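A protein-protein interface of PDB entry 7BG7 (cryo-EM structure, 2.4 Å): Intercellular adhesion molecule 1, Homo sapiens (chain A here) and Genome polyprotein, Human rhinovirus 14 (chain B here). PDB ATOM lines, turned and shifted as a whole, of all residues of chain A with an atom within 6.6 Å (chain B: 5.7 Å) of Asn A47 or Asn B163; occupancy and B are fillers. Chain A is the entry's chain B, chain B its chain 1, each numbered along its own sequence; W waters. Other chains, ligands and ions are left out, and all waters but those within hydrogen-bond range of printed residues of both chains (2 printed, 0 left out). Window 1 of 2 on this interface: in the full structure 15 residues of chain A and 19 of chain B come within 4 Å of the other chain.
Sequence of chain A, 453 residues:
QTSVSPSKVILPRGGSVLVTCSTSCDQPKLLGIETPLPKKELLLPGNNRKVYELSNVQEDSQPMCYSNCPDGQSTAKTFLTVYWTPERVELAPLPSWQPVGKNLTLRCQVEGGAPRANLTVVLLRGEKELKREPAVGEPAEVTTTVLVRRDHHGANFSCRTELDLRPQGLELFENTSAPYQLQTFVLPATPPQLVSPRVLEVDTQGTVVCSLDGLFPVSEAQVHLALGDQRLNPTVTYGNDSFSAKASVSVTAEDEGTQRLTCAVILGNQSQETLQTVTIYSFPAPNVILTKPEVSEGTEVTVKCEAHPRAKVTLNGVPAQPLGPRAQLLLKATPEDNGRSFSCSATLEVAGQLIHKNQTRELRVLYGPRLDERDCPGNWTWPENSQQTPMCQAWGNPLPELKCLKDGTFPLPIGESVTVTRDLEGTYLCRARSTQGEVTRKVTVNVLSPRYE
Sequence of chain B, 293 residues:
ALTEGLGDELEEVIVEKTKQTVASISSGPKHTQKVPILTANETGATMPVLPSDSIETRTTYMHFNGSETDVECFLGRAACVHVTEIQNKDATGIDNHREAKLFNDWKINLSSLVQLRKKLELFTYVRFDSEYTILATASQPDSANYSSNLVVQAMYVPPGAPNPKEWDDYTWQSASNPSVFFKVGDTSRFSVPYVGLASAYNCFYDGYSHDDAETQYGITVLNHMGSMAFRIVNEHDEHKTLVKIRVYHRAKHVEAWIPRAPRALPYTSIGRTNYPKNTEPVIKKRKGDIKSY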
ATOM      1  N   THR A  23     -18.709 -11.224 -26.336  1.00  0.00           N
ATOM      2  CA  THR A  23     -19.756 -11.466 -25.357  1.00  0.00           C
ATOM      3  C   THR A  23     -20.652 -10.246 -25.253  1.00  0.00           C
ATOM      4  O   THR A  23     -20.262  -9.141 -25.640  1.00  0.00           O
ATOM      5  CB  THR A  23     -19.182 -11.770 -23.964  1.00  0.00           C
ATOM      6  OG1 THR A  23     -18.339 -10.690 -23.547  1.00  0.00           O
ATOM      7  CG2 THR A  23     -18.386 -13.053 -23.959  1.00  0.00           C
ATOM      8  N   CYS A  25     -21.773  -9.723 -22.063  1.00  0.00           N
ATOM      9  CA  CYS A  25     -21.153  -9.309 -20.814  1.00  0.00           C
ATOM     10  C   CYS A  25     -20.006  -8.354 -21.110  1.00  0.00           C
ATOM     11  O   CYS A  25     -19.170  -8.617 -21.980  1.00  0.00           O
ATOM     12  CB  CYS A  25     -20.637 -10.527 -20.045  1.00  0.00           C
ATOM     13  SG  CYS A  25     -21.908 -11.517 -19.212  1.00  0.00           S
ATOM     14  N   ASP A  26     -19.972  -7.232 -20.396  1.00  0.00           N
ATOM     15  CA  ASP A  26     -18.882  -6.284 -20.591  1.00  0.00           C
ATOM     16  C   ASP A  26     -17.576  -6.825 -20.026  1.00  0.00           C
ATOM     17  O   ASP A  26     -16.511  -6.627 -20.619  1.00  0.00           O
ATOM     18  CB  ASP A  26     -19.233  -4.944 -19.950  1.00  0.00           C
ATOM     19  CG  ASP A  26     -20.316  -4.205 -20.704  1.00  0.00           C
ATOM     20  OD1 ASP A  26     -20.596  -4.579 -21.864  1.00  0.00           O
ATOM     21  OD2 ASP A  26     -20.897  -3.253 -20.136  1.00  0.00           O
ATOM     22  N   GLN A  27     -17.639  -7.521 -18.892  1.00  0.00           N
ATOM     23  CA  GLN A  27     -16.455  -8.006 -18.183  1.00  0.00           C
ATOM     24  C   GLN A  27     -16.564  -9.516 -18.011  1.00  0.00           C
ATOM     25  O   GLN A  27     -16.907 -10.003 -16.926  1.00  0.00           O
ATOM     26  CB  GLN A  27     -16.314  -7.317 -16.825  1.00  0.00           C
ATOM     27  CG  GLN A  27     -16.276  -5.799 -16.885  1.00  0.00           C
ATOM     28  CD  GLN A  27     -15.230  -5.280 -17.842  1.00  0.00           C
ATOM     29  OE1 GLN A  27     -14.137  -5.833 -17.938  1.00  0.00           O
ATOM     30  NE2 GLN A  27     -15.561  -4.217 -18.564  1.00  0.00           N
ATOM     31  N   PRO A  28     -16.252 -10.291 -19.051  1.00  0.00           N
ATOM     32  CA  PRO A  28     -16.169 -11.748 -18.887  1.00  0.00           C
ATOM     33  C   PRO A  28     -14.829 -12.190 -18.313  1.00  0.00           C
ATOM     34  O   PRO A  28     -13.793 -11.574 -18.564  1.00  0.00           O
ATOM     35  CB  PRO A  28     -16.363 -12.274 -20.311  1.00  0.00           C
ATOM     36  CG  PRO A  28     -15.832 -11.195 -21.175  1.00  0.00           C
ATOM     37  CD  PRO A  28     -16.035  -9.888 -20.451  1.00  0.00           C
ATOM     38  N   LYS A  29     -14.861 -13.275 -17.542  1.00  0.00           N
ATOM     39  CA  LYS A  29     -13.640 -13.812 -16.953  1.00  0.00           C
ATOM     40  C   LYS A  29     -12.986 -14.815 -17.886  1.00  0.00           C
ATOM     41  O   LYS A  29     -11.763 -14.806 -18.062  1.00  0.00           O
ATOM     42  CB  LYS A  29     -13.944 -14.459 -15.606  1.00  0.00           C
ATOM     43  CG  LYS A  29     -14.205 -13.462 -14.514  1.00  0.00           C
ATOM     44  CD  LYS A  29     -14.630 -14.143 -13.231  1.00  0.00           C
ATOM     45  CE  LYS A  29     -14.976 -13.119 -12.172  1.00  0.00           C
ATOM     46  NZ  LYS A  29     -16.162 -12.314 -12.564  1.00  0.00           N
ATOM     47  N   LEU A  31     -13.025 -16.045 -21.779  1.00  0.00           N
ATOM     48  CA  LEU A  31     -13.432 -15.770 -23.148  1.00  0.00           C
ATOM     49  C   LEU A  31     -12.330 -16.267 -24.063  1.00  0.00           C
ATOM     50  O   LEU A  31     -11.184 -15.827 -23.950  1.00  0.00           O
ATOM     51  CB  LEU A  31     -13.677 -14.277 -23.378  1.00  0.00           C
ATOM     52  CG  LEU A  31     -14.065 -13.854 -24.798  1.00  0.00           C
ATOM     53  CD1 LEU A  31     -15.392 -14.452 -25.206  1.00  0.00           C
ATOM     54  CD2 LEU A  31     -14.104 -12.347 -24.904  1.00  0.00           C
ATOM     55  N   LEU A  44      -5.483  -6.723 -28.866  1.00  0.00           N
ATOM     56  CA  LEU A  44      -6.668  -5.892 -28.987  1.00  0.00           C
ATOM     57  C   LEU A  44      -7.103  -5.458 -27.592  1.00  0.00           C
ATOM     58  O   LEU A  44      -7.157  -6.292 -26.677  1.00  0.00           O
ATOM     59  CB  LEU A  44      -7.804  -6.654 -29.677  1.00  0.00           C
ATOM     60  CG  LEU A  44      -9.046  -5.864 -30.080  1.00  0.00           C
ATOM     61  CD1 LEU A  44      -8.762  -5.012 -31.301  1.00  0.00           C
ATOM     62  CD2 LEU A  44     -10.200  -6.814 -30.349  1.00  0.00           C
ATOM     63  N   PRO A  45      -7.414  -4.178 -27.392  1.00  0.00           N
ATOM     64  CA  PRO A  45      -7.849  -3.730 -26.065  1.00  0.00           C
ATOM     65  C   PRO A  45      -9.280  -4.137 -25.761  1.00  0.00           C
ATOM     66  O   PRO A  45     -10.105  -4.311 -26.659  1.00  0.00           O
ATOM     67  CB  PRO A  45      -7.719  -2.206 -26.149  1.00  0.00           C
ATOM     68  CG  PRO A  45      -7.931  -1.905 -27.584  1.00  0.00           C
ATOM     69  CD  PRO A  45      -7.370  -3.064 -28.355  1.00  0.00           C
ATOM     70  N   GLY A  46      -9.570  -4.295 -24.474  1.00  0.00           N
ATOM     71  CA  GLY A  46     -10.905  -4.666 -24.062  1.00  0.00           C
ATOM     72  C   GLY A  46     -10.970  -6.080 -23.507  1.00  0.00           C
ATOM     73  O   GLY A  46     -10.033  -6.873 -23.620  1.00  0.00           O
ATOM     74  N   ASN A  47     -12.116  -6.398 -22.907  1.00  0.00           N
ATOM     75  CA  ASN A  47     -12.302  -7.649 -22.190  1.00  0.00           C
ATOM     76  C   ASN A  47     -13.321  -8.557 -22.857  1.00  0.00           C
ATOM     77  O   ASN A  47     -13.220  -9.778 -22.717  1.00  0.00           O
ATOM     78  CB  ASN A  47     -12.763  -7.431 -20.739  1.00  0.00           C
ATOM     79  CG  ASN A  47     -11.799  -6.587 -19.930  1.00  0.00           C
ATOM     80  OD1 ASN A  47     -11.144  -7.072 -19.006  1.00  0.00           O
ATOM     81  ND2 ASN A  47     -11.718  -5.310 -20.272  1.00  0.00           N
ATOM     82  N   ASN A  48     -14.288  -7.991 -23.579  1.00  0.00           N
ATOM     83  CA  ASN A  48     -15.472  -8.714 -24.013  1.00  0.00           C
ATOM     84  C   ASN A  48     -15.410  -9.128 -25.479  1.00  0.00           C
ATOM     85  O   ASN A  48     -16.365  -9.727 -25.977  1.00  0.00           O
ATOM     86  CB  ASN A  48     -16.721  -7.863 -23.774  1.00  0.00           C
ATOM     87  CG  ASN A  48     -16.749  -6.618 -24.627  1.00  0.00           C
ATOM     88  OD1 ASN A  48     -15.719  -6.167 -25.118  1.00  0.00           O
ATOM     89  ND2 ASN A  48     -17.934  -6.065 -24.822  1.00  0.00           N
ATOM     90  N   ARG A  49     -14.315  -8.829 -26.175  1.00  0.00           N
ATOM     91  CA  ARG A  49     -14.128  -9.211 -27.569  1.00  0.00           C
ATOM     92  C   ARG A  49     -12.685  -9.635 -27.780  1.00  0.00           C
ATOM     93  O   ARG A  49     -11.762  -8.955 -27.328  1.00  0.00           O
ATOM     94  CB  ARG A  49     -14.476  -8.070 -28.533  1.00  0.00           C
ATOM     95  CG  ARG A  49     -14.415  -8.492 -30.002  1.00  0.00           C
ATOM     96  CD  ARG A  49     -14.980  -7.434 -30.934  1.00  0.00           C
ATOM     97  NE  ARG A  49     -14.168  -6.223 -30.965  1.00  0.00           N
ATOM     98  CZ  ARG A  49     -13.207  -5.971 -31.851  1.00  0.00           C
ATOM     99  NH1 ARG A  49     -12.916  -6.844 -32.804  1.00  0.00           N
ATOM    100  NH2 ARG A  49     -12.533  -4.831 -31.780  1.00  0.00           N
ATOM    101  N   LYS A  50     -12.496 -10.749 -28.479  1.00  0.00           N
ATOM    102  CA  LYS A  50     -11.174 -11.244 -28.830  1.00  0.00           C
ATOM    103  C   LYS A  50     -11.153 -11.606 -30.305  1.00  0.00           C
ATOM    104  O   LYS A  50     -12.188 -11.968 -30.871  1.00  0.00           O
ATOM    105  CB  LYS A  50     -10.806 -12.464 -27.990  1.00  0.00           C
ATOM    106  CG  LYS A  50     -10.373 -12.133 -26.587  1.00  0.00           C
ATOM    107  CD  LYS A  50     -10.210 -13.387 -25.765  1.00  0.00           C
ATOM    108  CE  LYS A  50      -9.415 -13.130 -24.509  1.00  0.00           C
ATOM    109  NZ  LYS A  50     -10.072 -12.136 -23.625  1.00  0.00           N
ATOM    110  N   ASP B 105      -1.645  -6.492 -20.955  1.00  0.00           N
ATOM    111  CA  ASP B 105      -2.226  -7.150 -19.801  1.00  0.00           C
ATOM    112  C   ASP B 105      -2.073  -8.658 -19.945  1.00  0.00           C
ATOM    113  O   ASP B 105      -1.776  -9.178 -21.021  1.00  0.00           O
ATOM    114  CB  ASP B 105      -3.689  -6.754 -19.613  1.00  0.00           C
ATOM    115  CG  ASP B 105      -4.608  -7.472 -20.552  1.00  0.00           C
ATOM    116  OD1 ASP B 105      -4.399  -7.362 -21.774  1.00  0.00           O
ATOM    117  OD2 ASP B 105      -5.548  -8.136 -20.069  1.00  0.00           O
ATOM    118  N   VAL B 157      -5.137  -6.119 -11.528  1.00  0.00           N
ATOM    119  CA  VAL B 157      -6.583  -5.958 -11.650  1.00  0.00           C
ATOM    120  C   VAL B 157      -7.249  -7.186 -11.034  1.00  0.00           C
ATOM    121  O   VAL B 157      -6.861  -8.314 -11.369  1.00  0.00           O
ATOM    122  CB  VAL B 157      -7.022  -5.769 -13.114  1.00  0.00           C
ATOM    123  CG1 VAL B 157      -6.140  -4.756 -13.811  1.00  0.00           C
ATOM    124  CG2 VAL B 157      -6.992  -7.044 -13.826  1.00  0.00           C
ATOM    125  N   GLY B 160     -11.863 -10.409 -13.203  1.00  0.00           N
ATOM    126  CA  GLY B 160     -13.051  -9.935 -13.870  1.00  0.00           C
ATOM    127  C   GLY B 160     -13.153  -8.430 -13.966  1.00  0.00           C
ATOM    128  O   GLY B 160     -14.089  -7.930 -14.598  1.00  0.00           O
ATOM    129  N   ALA B 161     -12.226  -7.695 -13.361  1.00  0.00           N
ATOM    130  CA  ALA B 161     -12.243  -6.246 -13.434  1.00  0.00           C
ATOM    131  C   ALA B 161     -11.812  -5.786 -14.826  1.00  0.00           C
ATOM    132  O   ALA B 161     -11.068  -6.485 -15.517  1.00  0.00           O
ATOM    133  CB  ALA B 161     -11.325  -5.646 -12.375  1.00  0.00           C
ATOM    134  N   PRO B 162     -12.272  -4.619 -15.268  1.00  0.00           N
ATOM    135  CA  PRO B 162     -11.915  -4.156 -16.615  1.00  0.00           C
ATOM    136  C   PRO B 162     -10.432  -3.835 -16.742  1.00  0.00           C
ATOM    137  O   PRO B 162      -9.854  -3.143 -15.902  1.00  0.00           O
ATOM    138  CB  PRO B 162     -12.781  -2.905 -16.802  1.00  0.00           C
ATOM    139  CG  PRO B 162     -13.078  -2.442 -15.434  1.00  0.00           C
ATOM    140  CD  PRO B 162     -13.150  -3.660 -14.576  1.00  0.00           C
ATOM    141  N   ASN B 163      -9.824  -4.349 -17.804  1.00  0.00           N
ATOM    142  CA  ASN B 163      -8.452  -4.021 -18.136  1.00  0.00           C
ATOM    143  C   ASN B 163      -8.412  -2.686 -18.870  1.00  0.00           C
ATOM    144  O   ASN B 163      -9.380  -2.305 -19.530  1.00  0.00           O
ATOM    145  CB  ASN B 163      -7.794  -5.117 -18.967  1.00  0.00           C
ATOM    146  CG  ASN B 163      -7.842  -6.468 -18.297  1.00  0.00           C
ATOM    147  OD1 ASN B 163      -7.177  -6.701 -17.290  1.00  0.00           O
ATOM    148  ND2 ASN B 163      -8.619  -7.378 -18.865  1.00  0.00           N
ATOM    149  N   PRO B 164      -7.310  -1.950 -18.762  1.00  0.00           N
ATOM    150  CA  PRO B 164      -7.184  -0.715 -19.541  1.00  0.00           C
ATOM    151  C   PRO B 164      -7.265  -0.978 -21.034  1.00  0.00           C
ATOM    152  O   PRO B 164      -6.808  -2.004 -21.534  1.00  0.00           O
ATOM    153  CB  PRO B 164      -5.801  -0.191 -19.145  1.00  0.00           C
ATOM    154  CG  PRO B 164      -5.540  -0.794 -17.825  1.00  0.00           C
ATOM    155  CD  PRO B 164      -6.144  -2.150 -17.890  1.00  0.00           C
ATOM    156  N   LYS B 165      -7.869  -0.031 -21.746  1.00  0.00           N
ATOM    157  CA  LYS B 165      -8.107  -0.167 -23.171  1.00  0.00           C
ATOM    158  C   LYS B 165      -7.179   0.699 -24.003  1.00  0.00           C
ATOM    159  O   LYS B 165      -7.015   0.435 -25.195  1.00  0.00           O
ATOM    160  CB  LYS B 165      -9.560   0.191 -23.508  1.00  0.00           C
ATOM    161  CG  LYS B 165     -10.571  -0.752 -22.891  1.00  0.00           C
ATOM    162  CD  LYS B 165     -11.989  -0.357 -23.242  1.00  0.00           C
ATOM    163  CE  LYS B 165     -12.988  -1.298 -22.594  1.00  0.00           C
ATOM    164  NZ  LYS B 165     -14.399  -0.927 -22.889  1.00  0.00           N
ATOM    165  N   ASP B 169      -5.644   5.473 -20.476  1.00  0.00           N
ATOM    166  CA  ASP B 169      -7.011   5.301 -20.012  1.00  0.00           C
ATOM    167  C   ASP B 169      -7.129   5.643 -18.524  1.00  0.00           C
ATOM    168  O   ASP B 169      -6.159   5.589 -17.765  1.00  0.00           O
ATOM    169  CB  ASP B 169      -7.451   3.858 -20.263  1.00  0.00           C
ATOM    170  CG  ASP B 169      -8.904   3.618 -19.941  1.00  0.00           C
ATOM    171  OD1 ASP B 169      -9.623   4.588 -19.624  1.00  0.00           O
ATOM    172  OD2 ASP B 169      -9.330   2.449 -20.002  1.00  0.00           O
ATOM    173  N   THR B 171      -8.582   3.841 -16.449  1.00  0.00           N
ATOM    174  CA  THR B 171      -8.493   2.606 -15.682  1.00  0.00           C
ATOM    175  C   THR B 171      -7.183   2.534 -14.916  1.00  0.00           C
ATOM    176  O   THR B 171      -7.120   1.912 -13.853  1.00  0.00           O
ATOM    177  CB  THR B 171      -8.633   1.396 -16.605  1.00  0.00           C
ATOM    178  OG1 THR B 171      -9.868   1.484 -17.325  1.00  0.00           O
ATOM    179  CG2 THR B 171      -8.604   0.112 -15.804  1.00  0.00           C
ATOM    180  N   SER B 227      -5.136 -10.550 -12.760  1.00  0.00           N
ATOM    181  CA  SER B 227      -4.521 -10.168 -14.023  1.00  0.00           C
ATOM    182  C   SER B 227      -3.594  -8.992 -13.755  1.00  0.00           C
ATOM    183  O   SER B 227      -3.762  -8.275 -12.767  1.00  0.00           O
ATOM    184  CB  SER B 227      -5.574  -9.821 -15.081  1.00  0.00           C
ATOM    185  OG  SER B 227      -5.011  -9.767 -16.373  1.00  0.00           O
ATOM    186  N   ALA B 229      -1.706  -5.624 -15.632  1.00  0.00           N
ATOM    187  CA  ALA B 229      -1.557  -4.713 -16.754  1.00  0.00           C
ATOM    188  C   ALA B 229      -0.273  -3.923 -16.569  1.00  0.00           C
ATOM    189  O   ALA B 229       0.093  -3.577 -15.445  1.00  0.00           O
ATOM    190  CB  ALA B 229      -2.755  -3.775 -16.874  1.00  0.00           C
HETATM  191  O   HOH W   1     -13.237  -9.091 -16.785  1.00  0.00           O
HETATM  192  O   HOH W   2      -6.755  -4.591 -22.442  1.00  0.00           O
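The side-chain amide nitrogen of Asn B163 lies within hydrogen-bond range of the side-chain amide oxygen of Asn A47 (2.5 Å).
The side-chain amide oxygen (OE1) of Gln A27 sits close to the backbone nitrogen (N) of Pro B162, at 3.5 Å.
The side-chain carboxylate (OD2) of Asp B105 lies close to the side-chain amide nitrogen (ND2) of Asn B163 (3.4 Å).
The backbone NH (N) of Lys B165 lies within hydrogen-bond range of the side-chain carboxylate (OD2) of Asp B169 (3.4 Å).
The side-chain amide oxygen (OE1) of Gln A27 sits close to the side-chain amide nitrogen (ND2) of Asn A47 (3.4 Å).
Among the printed residues, merely in contact across the chains: Gln A27 with Gly B160, Gln A27 with Ala B161, Lys A29 with Gly B160, Pro A45 with Lys B165, Asn A47 with Ala B161 and Asn A47 with Pro B162.
Asn A47 touches three residues of chain B.
Printed residues of chain A within 4 Å of Ala B161: Gln A27 (3.9 Å) and Asn A47 (3.5 Å).
Of the printed residues of chain A, Pro B162 touches Gln A27 (3.1 Å) and Asn A47 (3.8 Å).
Of the printed residues of chain A, Asn B163 touches Asn A47 (2.5 Å).
Printed residues of chain A within 4 Å of Lys B165: Pro A45.
Of the 14 printed residues of chain A, 4 touch a printed residue of chain B.
Hydrophobic or aromatic side chains of chain A that line the printed part of chain B: Pro A45.
Among the printed residues, no Asp or Glu carboxylate lies within 4 Å of a Lys or Arg side-chain nitrogen of the other chain.
Water W1 lies within hydrogen-bond range of O of Gly B160 (2.6 Å) and O of Pro A28 (3.1 Å).
Water W2 lies within hydrogen-bond range of the backbone carbonyl oxygen (O) of Pro B164 and the backbone NH (N) of Gly A46.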
